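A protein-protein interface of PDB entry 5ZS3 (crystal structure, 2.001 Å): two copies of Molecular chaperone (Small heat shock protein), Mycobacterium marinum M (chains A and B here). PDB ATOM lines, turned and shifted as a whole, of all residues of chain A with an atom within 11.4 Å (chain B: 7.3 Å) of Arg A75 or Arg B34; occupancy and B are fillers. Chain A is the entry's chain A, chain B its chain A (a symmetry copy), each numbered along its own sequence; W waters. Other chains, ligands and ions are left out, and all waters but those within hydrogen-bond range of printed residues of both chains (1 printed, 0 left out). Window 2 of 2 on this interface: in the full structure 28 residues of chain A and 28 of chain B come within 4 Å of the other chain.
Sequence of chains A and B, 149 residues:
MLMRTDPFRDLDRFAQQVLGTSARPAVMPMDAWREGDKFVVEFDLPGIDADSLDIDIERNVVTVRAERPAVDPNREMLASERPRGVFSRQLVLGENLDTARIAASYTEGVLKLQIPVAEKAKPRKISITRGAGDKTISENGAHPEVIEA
NH1 of Arg A75 is in hydrogen-bond range of O of Arg B34, at 3.4 Å.
The backbone NH (N) of Ala B32 lies within hydrogen-bond range of the backbone carbonyl oxygen (O) of Ala A79 (2.9 Å).
The backbone NH (N) of Leu A78 lies within hydrogen-bond range of the backbone carbonyl oxygen (O) of Ala B32, at 2.9 Å.
NE of Arg B34 lies within hydrogen-bond range of O of Gly B36, 2.8 Å away.
NH2 of Arg B34 is in salt-bridge range of OE2 of Glu B119, 3.3 Å away.
O of Trp B33 lies within hydrogen-bond range of N of Val B40 (2.8 Å).
NE1 of Trp B33 sits at hydrogen-bond distance from OE2 of Glu B35, 2.8 Å away.
Arg A75 touches Trp B33 (NH1 to CD1, 3.8 Å).
NH1 of Arg A75 touches CG of Glu B35, 3.9 Å away.
Met A77 touches Ala B32 (C to O, 3.8 Å).
Trp B33 touches Met A77 (CB to SD, 3.8 Å).
Phe B39 touches Leu A78 (CE1 to CD1, 3.999 Å).
Of the printed residues of chain B, Arg A75 touches Trp B33, Arg B34 and Glu B35.
Of chain A, only Arg A75 (3.8 Å) and Met A77 (3.8 Å) come within 4 Å of Trp B33.
Glu B35 touches just one residue of chain A: Arg A75 (3.9 Å).
No residue of chain A comes within 4 Å of Gly B36.
No residue of chain A comes within 4 Å of Val B117.
Printed residues of chain B within 4 Å of Leu A78: Ala B32 (2.9 Å) and Phe B39 (3.999 Å).
Of the printed residues of chain B, Ala A79 touches Ala B32.
Of the printed residues of chain A, Phe B39 touches Leu A78.
Asn A74 touches none of the printed residues of chain B.
Asn B96 touches none of the printed residues of chain A.
The nearest residue of chain B that does not touch Arg A75 is Gly B36 (5.7 Å).
The nearest residue of chain A that does not touch Arg B34 is Glu A76 (4.9 Å).
Along chain B the printed residues that touch a printed residue of chain A span positions 32 to 39.
Among the printed residues, 8 pairs touch across the chains.
Among the printed residues, no Asp or Glu carboxylate lies within 4 Å of a Lys or Arg side-chain nitrogen of the other chain.
No position is printed for both chains.
Of the 8 pairs that touch across the chains among the printed residues, none has its exchanged pair printed and touching as well.
Water W1 lies within hydrogen-bond range of the backbone carbonyl oxygen of Arg B34 (2.8 Å), the guanidinium group of Arg A75 (2.9 Å) and the backbone carbonyl oxygen of Glu A76 (3.1 Å).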
ATOM      1  N   PRO A  69     -16.974   2.945 -33.458  1.00  0.00           N
ATOM      2  CA  PRO A  69     -18.209   3.161 -32.694  1.00  0.00           C
ATOM      3  C   PRO A  69     -17.987   3.016 -31.192  1.00  0.00           C
ATOM      4  O   PRO A  69     -17.131   2.259 -30.732  1.00  0.00           O
ATOM      5  CB  PRO A  69     -19.144   2.062 -33.217  1.00  0.00           C
ATOM      6  CG  PRO A  69     -18.219   1.029 -33.843  1.00  0.00           C
ATOM      7  CD  PRO A  69     -17.093   1.845 -34.425  1.00  0.00           C
ATOM      8  N   ALA A  70     -18.758   3.781 -30.428  1.00  0.00           N
ATOM      9  CA  ALA A  70     -18.764   3.649 -28.984  1.00  0.00           C
ATOM     10  C   ALA A  70     -19.320   2.289 -28.598  1.00  0.00           C
ATOM     11  O   ALA A  70     -20.102   1.680 -29.331  1.00  0.00           O
ATOM     12  CB  ALA A  70     -19.613   4.751 -28.346  1.00  0.00           C
ATOM     13  N   VAL A  71     -18.914   1.812 -27.424  1.00  0.00           N
ATOM     14  CA  VAL A  71     -19.417   0.537 -26.932  1.00  0.00           C
ATOM     15  C   VAL A  71     -20.885   0.695 -26.562  1.00  0.00           C
ATOM     16  O   VAL A  71     -21.300   1.730 -26.014  1.00  0.00           O
ATOM     17  CB  VAL A  71     -18.582   0.064 -25.730  1.00  0.00           C
ATOM     18  CG1 VAL A  71     -19.261  -1.100 -25.031  1.00  0.00           C
ATOM     19  CG2 VAL A  71     -17.182  -0.327 -26.183  1.00  0.00           C
ATOM     20  N   ASP A  72     -21.692  -0.313 -26.909  1.00  0.00           N
ATOM     21  CA  ASP A  72     -23.079  -0.427 -26.469  1.00  0.00           C
ATOM     22  C   ASP A  72     -23.207  -0.043 -25.000  1.00  0.00           C
ATOM     23  O   ASP A  72     -22.649  -0.730 -24.137  1.00  0.00           O
ATOM     24  CB  ASP A  72     -23.565  -1.857 -26.678  1.00  0.00           C
ATOM     25  CG  ASP A  72     -25.034  -2.051 -26.320  1.00  0.00           C
ATOM     26  OD1 ASP A  72     -25.565  -1.340 -25.434  1.00  0.00           O
ATOM     27  OD2 ASP A  72     -25.644  -2.972 -26.905  1.00  0.00           O
ATOM     28  N   PRO A  73     -23.939   1.028 -24.680  1.00  0.00           N
ATOM     29  CA  PRO A  73     -24.066   1.447 -23.273  1.00  0.00           C
ATOM     30  C   PRO A  73     -24.580   0.363 -22.354  1.00  0.00           C
ATOM     31  O   PRO A  73     -24.322   0.422 -21.143  1.00  0.00           O
ATOM     32  CB  PRO A  73     -25.070   2.608 -23.342  1.00  0.00           C
ATOM     33  CG  PRO A  73     -25.097   3.027 -24.774  1.00  0.00           C
ATOM     34  CD  PRO A  73     -24.801   1.811 -25.578  1.00  0.00           C
ATOM     35  N   ASN A  74     -25.274  -0.641 -22.884  1.00  0.00           N
ATOM     36  CA  ASN A  74     -25.803  -1.717 -22.064  1.00  0.00           C
ATOM     37  C   ASN A  74     -24.788  -2.823 -21.832  1.00  0.00           C
ATOM     38  O   ASN A  74     -25.111  -3.820 -21.177  1.00  0.00           O
ATOM     39  CB  ASN A  74     -27.066  -2.294 -22.703  1.00  0.00           C
ATOM     40  CG  ASN A  74     -28.290  -1.485 -22.370  1.00  0.00           C
ATOM     41  OD1 ASN A  74     -28.455  -1.031 -21.234  1.00  0.00           O
ATOM     42  ND2 ASN A  74     -29.156  -1.289 -23.358  1.00  0.00           N
ATOM     43  N   ARG A  75     -23.583  -2.686 -22.357  1.00  0.00           N
ATOM     44  CA  ARG A  75     -22.558  -3.701 -22.206  1.00  0.00           C
ATOM     45  C   ARG A  75     -21.642  -3.298 -21.057  1.00  0.00           C
ATOM     46  O   ARG A  75     -21.052  -2.217 -21.086  1.00  0.00           O
ATOM     47  CB  ARG A  75     -21.797  -3.853 -23.519  1.00  0.00           C
ATOM     48  CG  ARG A  75     -20.426  -4.405 -23.366  1.00  0.00           C
ATOM     49  CD  ARG A  75     -20.518  -5.879 -23.358  1.00  0.00           C
ATOM     50  NE  ARG A  75     -21.148  -6.378 -24.571  1.00  0.00           N
ATOM     51  CZ  ARG A  75     -21.646  -7.602 -24.638  1.00  0.00           C
ATOM     52  NH1 ARG A  75     -21.558  -8.372 -23.566  1.00  0.00           N
ATOM     53  NH2 ARG A  75     -22.238  -8.052 -25.739  1.00  0.00           N
ATOM     54  N   GLU A  76     -21.514  -4.172 -20.059  1.00  0.00           N
ATOM     55  CA  GLU A  76     -20.587  -3.931 -18.954  1.00  0.00           C
ATOM     56  C   GLU A  76     -19.189  -4.366 -19.378  1.00  0.00           C
ATOM     57  O   GLU A  76     -18.899  -5.570 -19.462  1.00  0.00           O
ATOM     58  CB  GLU A  76     -21.051  -4.685 -17.704  1.00  0.00           C
ATOM     59  CG  GLU A  76     -20.037  -4.790 -16.567  1.00  0.00           C
ATOM     60  CD  GLU A  76     -20.670  -5.121 -15.199  1.00  0.00           C
ATOM     61  OE1 GLU A  76     -20.126  -5.991 -14.473  1.00  0.00           O
ATOM     62  OE2 GLU A  76     -21.709  -4.513 -14.851  1.00  0.00           O
ATOM     63  N   MET A  77     -18.312  -3.392 -19.616  1.00  0.00           N
ATOM     64  CA  MET A  77     -16.935  -3.714 -19.955  1.00  0.00           C
ATOM     65  C   MET A  77     -16.154  -3.904 -18.631  1.00  0.00           C
ATOM     66  O   MET A  77     -16.307  -3.126 -17.693  1.00  0.00           O
ATOM     67  CB  MET A  77     -16.299  -2.594 -20.806  1.00  0.00           C
ATOM     68  CG  MET A  77     -17.079  -2.225 -22.072  1.00  0.00           C
ATOM     69  SD  MET A  77     -16.944  -3.672 -23.315  1.00  0.00           S
ATOM     70  CE  MET A  77     -15.067  -3.308 -23.893  1.00  0.00           C
ATOM     71  N   LEU A  78     -15.280  -4.897 -18.574  1.00  0.00           N
ATOM     72  CA  LEU A  78     -14.316  -4.961 -17.474  1.00  0.00           C
ATOM     73  C   LEU A  78     -13.060  -4.120 -17.737  1.00  0.00           C
ATOM     74  O   LEU A  78     -12.411  -3.650 -16.796  1.00  0.00           O
ATOM     75  CB  LEU A  78     -13.951  -6.418 -17.185  1.00  0.00           C
ATOM     76  CG  LEU A  78     -15.219  -7.135 -16.716  1.00  0.00           C
ATOM     77  CD1 LEU A  78     -14.871  -8.530 -16.246  1.00  0.00           C
ATOM     78  CD2 LEU A  78     -16.051  -6.374 -15.645  1.00  0.00           C
ATOM     79  N   ALA A  79     -12.670  -3.929 -18.991  1.00  0.00           N
ATOM     80  CA  ALA A  79     -11.633  -2.962 -19.329  1.00  0.00           C
ATOM     81  C   ALA A  79     -12.072  -2.305 -20.621  1.00  0.00           C
ATOM     82  O   ALA A  79     -12.657  -2.973 -21.481  1.00  0.00           O
ATOM     83  CB  ALA A  79     -10.251  -3.625 -19.491  1.00  0.00           C
ATOM     84  N   SER A  80     -11.872  -0.987 -20.740  1.00  0.00           N
ATOM     85  CA  SER A  80     -12.266  -0.368 -22.018  1.00  0.00           C
ATOM     86  C   SER A  80     -11.265   0.756 -22.321  1.00  0.00           C
ATOM     87  O   SER A  80     -11.585   1.936 -22.377  1.00  0.00           O
ATOM     88  CB  SER A  80     -13.717   0.125 -21.998  1.00  0.00           C
ATOM     89  OG  SER A  80     -13.946   0.987 -20.905  1.00  0.00           O
ATOM     90  N   ARG A  82      -9.342   1.046 -25.127  1.00  0.00           N
ATOM     91  CA  ARG A  82      -9.069   1.365 -26.515  1.00  0.00           C
ATOM     92  C   ARG A  82      -9.808   2.645 -26.903  1.00  0.00           C
ATOM     93  O   ARG A  82     -10.962   2.843 -26.514  1.00  0.00           O
ATOM     94  CB  ARG A  82      -9.468   0.191 -27.412  1.00  0.00           C
ATOM     95  CG  ARG A  82      -8.582  -1.028 -27.154  1.00  0.00           C
ATOM     96  CD  ARG A  82      -9.212  -2.335 -27.543  1.00  0.00           C
ATOM     97  NE  ARG A  82      -9.235  -2.539 -28.983  1.00  0.00           N
ATOM     98  CZ  ARG A  82     -10.253  -3.076 -29.642  1.00  0.00           C
ATOM     99  NH1 ARG A  82     -11.345  -3.455 -28.996  1.00  0.00           N
ATOM    100  NH2 ARG A  82     -10.178  -3.213 -30.954  1.00  0.00           N
ATOM    101  N   ARG A  84     -12.024   5.335 -28.763  1.00  0.00           N
ATOM    102  CA  ARG A  84     -13.210   5.206 -29.595  1.00  0.00           C
ATOM    103  C   ARG A  84     -13.697   6.578 -30.039  1.00  0.00           C
ATOM    104  O   ARG A  84     -13.223   7.620 -29.564  1.00  0.00           O
ATOM    105  CB  ARG A  84     -14.308   4.447 -28.847  1.00  0.00           C
ATOM    106  CG  ARG A  84     -14.003   2.955 -28.854  1.00  0.00           C
ATOM    107  CD  ARG A  84     -14.956   2.125 -28.038  1.00  0.00           C
ATOM    108  NE  ARG A  84     -14.454   0.758 -27.990  1.00  0.00           N
ATOM    109  CZ  ARG A  84     -14.505  -0.097 -29.002  1.00  0.00           C
ATOM    110  NH1 ARG A  84     -15.096   0.243 -30.143  1.00  0.00           N
ATOM    111  NH2 ARG A  84     -14.000  -1.317 -28.856  1.00  0.00           N
ATOM    112  N   ALA B  32     -11.879  -5.621 -22.453  1.00  0.00           N
ATOM    113  CA  ALA B  32     -12.136  -6.973 -21.981  1.00  0.00           C
ATOM    114  C   ALA B  32     -13.578  -7.046 -21.522  1.00  0.00           C
ATOM    115  O   ALA B  32     -14.088  -6.100 -20.905  1.00  0.00           O
ATOM    116  CB  ALA B  32     -11.191  -7.353 -20.835  1.00  0.00           C
ATOM    117  N   TRP B  33     -14.262  -8.137 -21.836  1.00  0.00           N
ATOM    118  CA  TRP B  33     -15.652  -8.209 -21.394  1.00  0.00           C
ATOM    119  C   TRP B  33     -16.091  -9.662 -21.397  1.00  0.00           C
ATOM    120  O   TRP B  33     -15.508 -10.512 -22.077  1.00  0.00           O
ATOM    121  CB  TRP B  33     -16.586  -7.339 -22.264  1.00  0.00           C
ATOM    122  CG  TRP B  33     -16.732  -7.830 -23.658  1.00  0.00           C
ATOM    123  CD1 TRP B  33     -17.773  -8.558 -24.172  1.00  0.00           C
ATOM    124  CD2 TRP B  33     -15.800  -7.658 -24.723  1.00  0.00           C
ATOM    125  NE1 TRP B  33     -17.534  -8.854 -25.491  1.00  0.00           N
ATOM    126  CE2 TRP B  33     -16.334  -8.306 -25.857  1.00  0.00           C
ATOM    127  CE3 TRP B  33     -14.570  -7.008 -24.836  1.00  0.00           C
ATOM    128  CZ2 TRP B  33     -15.687  -8.314 -27.084  1.00  0.00           C
ATOM    129  CZ3 TRP B  33     -13.921  -7.023 -26.064  1.00  0.00           C
ATOM    130  CH2 TRP B  33     -14.479  -7.680 -27.165  1.00  0.00           C
ATOM    131  N   ARG B  34     -17.124  -9.940 -20.608  1.00  0.00           N
ATOM    132  CA  ARG B  34     -17.722 -11.257 -20.561  1.00  0.00           C
ATOM    133  C   ARG B  34     -18.905 -11.300 -21.517  1.00  0.00           C
ATOM    134  O   ARG B  34     -19.773 -10.427 -21.484  1.00  0.00           O
ATOM    135  CB  ARG B  34     -18.161 -11.583 -19.136  1.00  0.00           C
ATOM    136  CG  ARG B  34     -19.001 -12.822 -19.042  1.00  0.00           C
ATOM    137  CD  ARG B  34     -18.867 -13.500 -17.720  1.00  0.00           C
ATOM    138  NE  ARG B  34     -19.509 -14.805 -17.773  1.00  0.00           N
ATOM    139  CZ  ARG B  34     -19.565 -15.639 -16.747  1.00  0.00           C
ATOM    140  NH1 ARG B  34     -19.016 -15.283 -15.597  1.00  0.00           N
ATOM    141  NH2 ARG B  34     -20.166 -16.817 -16.871  1.00  0.00           N
ATOM    142  N   GLU B  35     -18.925 -12.311 -22.376  1.00  0.00           N
ATOM    143  CA  GLU B  35     -19.969 -12.510 -23.379  1.00  0.00           C
ATOM    144  C   GLU B  35     -20.589 -13.866 -23.092  1.00  0.00           C
ATOM    145  O   GLU B  35     -20.185 -14.866 -23.683  1.00  0.00           O
ATOM    146  CB  GLU B  35     -19.421 -12.468 -24.760  1.00  0.00           C
ATOM    147  CG  GLU B  35     -19.738 -11.213 -25.497  1.00  0.00           C
ATOM    148  CD  GLU B  35     -19.426 -11.338 -26.968  1.00  0.00           C
ATOM    149  OE1 GLU B  35     -19.861 -12.343 -27.575  1.00  0.00           O
ATOM    150  OE2 GLU B  35     -18.752 -10.438 -27.516  1.00  0.00           O
ATOM    151  N   GLY B  36     -21.531 -13.900 -22.150  1.00  0.00           N
ATOM    152  CA  GLY B  36     -22.166 -15.146 -21.764  1.00  0.00           C
ATOM    153  C   GLY B  36     -21.175 -16.127 -21.176  1.00  0.00           C
ATOM    154  O   GLY B  36     -20.677 -15.933 -20.061  1.00  0.00           O
ATOM    155  N   ASP B  37     -20.872 -17.184 -21.926  1.00  0.00           N
ATOM    156  CA  ASP B  37     -20.004 -18.256 -21.465  1.00  0.00           C
ATOM    157  C   ASP B  37     -18.560 -18.081 -21.918  1.00  0.00           C
ATOM    158  O   ASP B  37     -17.755 -19.007 -21.745  1.00  0.00           O
ATOM    159  CB  ASP B  37     -20.534 -19.602 -21.969  1.00  0.00           C
ATOM    160  CG  ASP B  37     -20.666 -19.646 -23.505  1.00  0.00           C
ATOM    161  OD1 ASP B  37     -20.602 -18.574 -24.154  1.00  0.00           O
ATOM    162  OD2 ASP B  37     -20.830 -20.754 -24.068  1.00  0.00           O
ATOM    163  N   LYS B  38     -18.205 -16.919 -22.478  1.00  0.00           N
ATOM    164  CA  LYS B  38     -16.849 -16.659 -22.936  1.00  0.00           C
ATOM    165  C   LYS B  38     -16.384 -15.327 -22.376  1.00  0.00           C
ATOM    166  O   LYS B  38     -17.172 -14.388 -22.240  1.00  0.00           O
ATOM    167  CB  LYS B  38     -16.749 -16.637 -24.480  1.00  0.00           C
ATOM    168  N   PHE B  39     -15.105 -15.255 -22.048  1.00  0.00           N
ATOM    169  CA  PHE B  39     -14.462 -13.995 -21.712  1.00  0.00           C
ATOM    170  C   PHE B  39     -13.633 -13.560 -22.913  1.00  0.00           C
ATOM    171  O   PHE B  39     -12.867 -14.356 -23.467  1.00  0.00           O
ATOM    172  CB  PHE B  39     -13.598 -14.151 -20.471  1.00  0.00           C
ATOM    173  CG  PHE B  39     -12.971 -12.877 -20.020  1.00  0.00           C
ATOM    174  CD1 PHE B  39     -13.762 -11.814 -19.622  1.00  0.00           C
ATOM    175  CD2 PHE B  39     -11.601 -12.740 -20.000  1.00  0.00           C
ATOM    176  CE1 PHE B  39     -13.185 -10.627 -19.204  1.00  0.00           C
ATOM    177  CE2 PHE B  39     -11.007 -11.543 -19.585  1.00  0.00           C
ATOM    178  CZ  PHE B  39     -11.804 -10.496 -19.188  1.00  0.00           C
ATOM    179  N   VAL B  40     -13.801 -12.312 -23.339  1.00  0.00           N
ATOM    180  CA  VAL B  40     -13.133 -11.837 -24.546  1.00  0.00           C
ATOM    181  C   VAL B  40     -12.238 -10.666 -24.180  1.00  0.00           C
ATOM    182  O   VAL B  40     -12.632  -9.777 -23.412  1.00  0.00           O
ATOM    183  CB  VAL B  40     -14.141 -11.436 -25.645  1.00  0.00           C
ATOM    184  CG1 VAL B  40     -13.416 -11.139 -26.937  1.00  0.00           C
ATOM    185  CG2 VAL B  40     -15.182 -12.544 -25.853  1.00  0.00           C
ATOM    186  N   ASN B  96     -12.256 -19.544 -12.861  1.00  0.00           N
ATOM    187  CA  ASN B  96     -13.311 -20.062 -13.727  1.00  0.00           C
ATOM    188  C   ASN B  96     -12.984 -19.949 -15.208  1.00  0.00           C
ATOM    189  O   ASN B  96     -13.834 -20.310 -16.030  1.00  0.00           O
ATOM    190  CB  ASN B  96     -14.634 -19.346 -13.461  1.00  0.00           C
ATOM    191  CG  ASN B  96     -15.259 -19.750 -12.148  1.00  0.00           C
ATOM    192  OD1 ASN B  96     -14.811 -20.699 -11.495  1.00  0.00           O
ATOM    193  ND2 ASN B  96     -16.314 -19.042 -11.757  1.00  0.00           N
ATOM    194  N   LEU B  97     -11.826 -19.419 -15.582  1.00  0.00           N
ATOM    195  CA  LEU B  97     -11.491 -19.265 -16.992  1.00  0.00           C
ATOM    196  C   LEU B  97     -10.697 -20.487 -17.435  1.00  0.00           C
ATOM    197  O   LEU B  97      -9.647 -20.797 -16.856  1.00  0.00           O
ATOM    198  CB  LEU B  97     -10.701 -17.986 -17.258  1.00  0.00           C
ATOM    199  CG  LEU B  97     -11.491 -16.694 -17.034  1.00  0.00           C
ATOM    200  CD1 LEU B  97     -10.934 -15.563 -17.853  1.00  0.00           C
ATOM    201  CD2 LEU B  97     -12.961 -16.880 -17.309  1.00  0.00           C
ATOM    202  N   VAL B 117     -15.585 -19.616 -20.161  1.00  0.00           N
ATOM    203  CA  VAL B 117     -15.803 -19.487 -18.731  1.00  0.00           C
ATOM    204  C   VAL B 117     -16.381 -20.801 -18.255  1.00  0.00           C
ATOM    205  O   VAL B 117     -17.345 -21.305 -18.838  1.00  0.00           O
ATOM    206  CB  VAL B 117     -16.749 -18.322 -18.401  1.00  0.00           C
ATOM    207  CG1 VAL B 117     -17.131 -18.375 -16.941  1.00  0.00           C
ATOM    208  CG2 VAL B 117     -16.104 -16.996 -18.743  1.00  0.00           C
ATOM    209  N   ALA B 118     -15.780 -21.372 -17.220  1.00  0.00           N
ATOM    210  CA  ALA B 118     -16.147 -22.699 -16.739  1.00  0.00           C
ATOM    211  C   ALA B 118     -16.460 -22.547 -15.259  1.00  0.00           C
ATOM    212  O   ALA B 118     -15.569 -22.698 -14.424  1.00  0.00           O
ATOM    213  CB  ALA B 118     -15.028 -23.705 -16.999  1.00  0.00           C
ATOM    214  N   GLU B 119     -17.696 -22.182 -14.935  1.00  0.00           N
ATOM    215  CA  GLU B 119     -18.029 -21.918 -13.543  1.00  0.00           C
ATOM    216  C   GLU B 119     -17.925 -23.206 -12.732  1.00  0.00           C
ATOM    217  O   GLU B 119     -18.300 -24.285 -13.202  1.00  0.00           O
ATOM    218  CB  GLU B 119     -19.435 -21.325 -13.429  1.00  0.00           C
ATOM    219  CG  GLU B 119     -19.739 -20.212 -14.425  1.00  0.00           C
ATOM    220  CD  GLU B 119     -19.793 -18.835 -13.780  1.00  0.00           C
ATOM    221  OE1 GLU B 119     -18.811 -18.451 -13.106  1.00  0.00           O
ATOM    222  OE2 GLU B 119     -20.818 -18.137 -13.955  1.00  0.00           O
HETATM  223  O   HOH W   1     -20.478  -7.821 -20.928  1.00  0.00           O
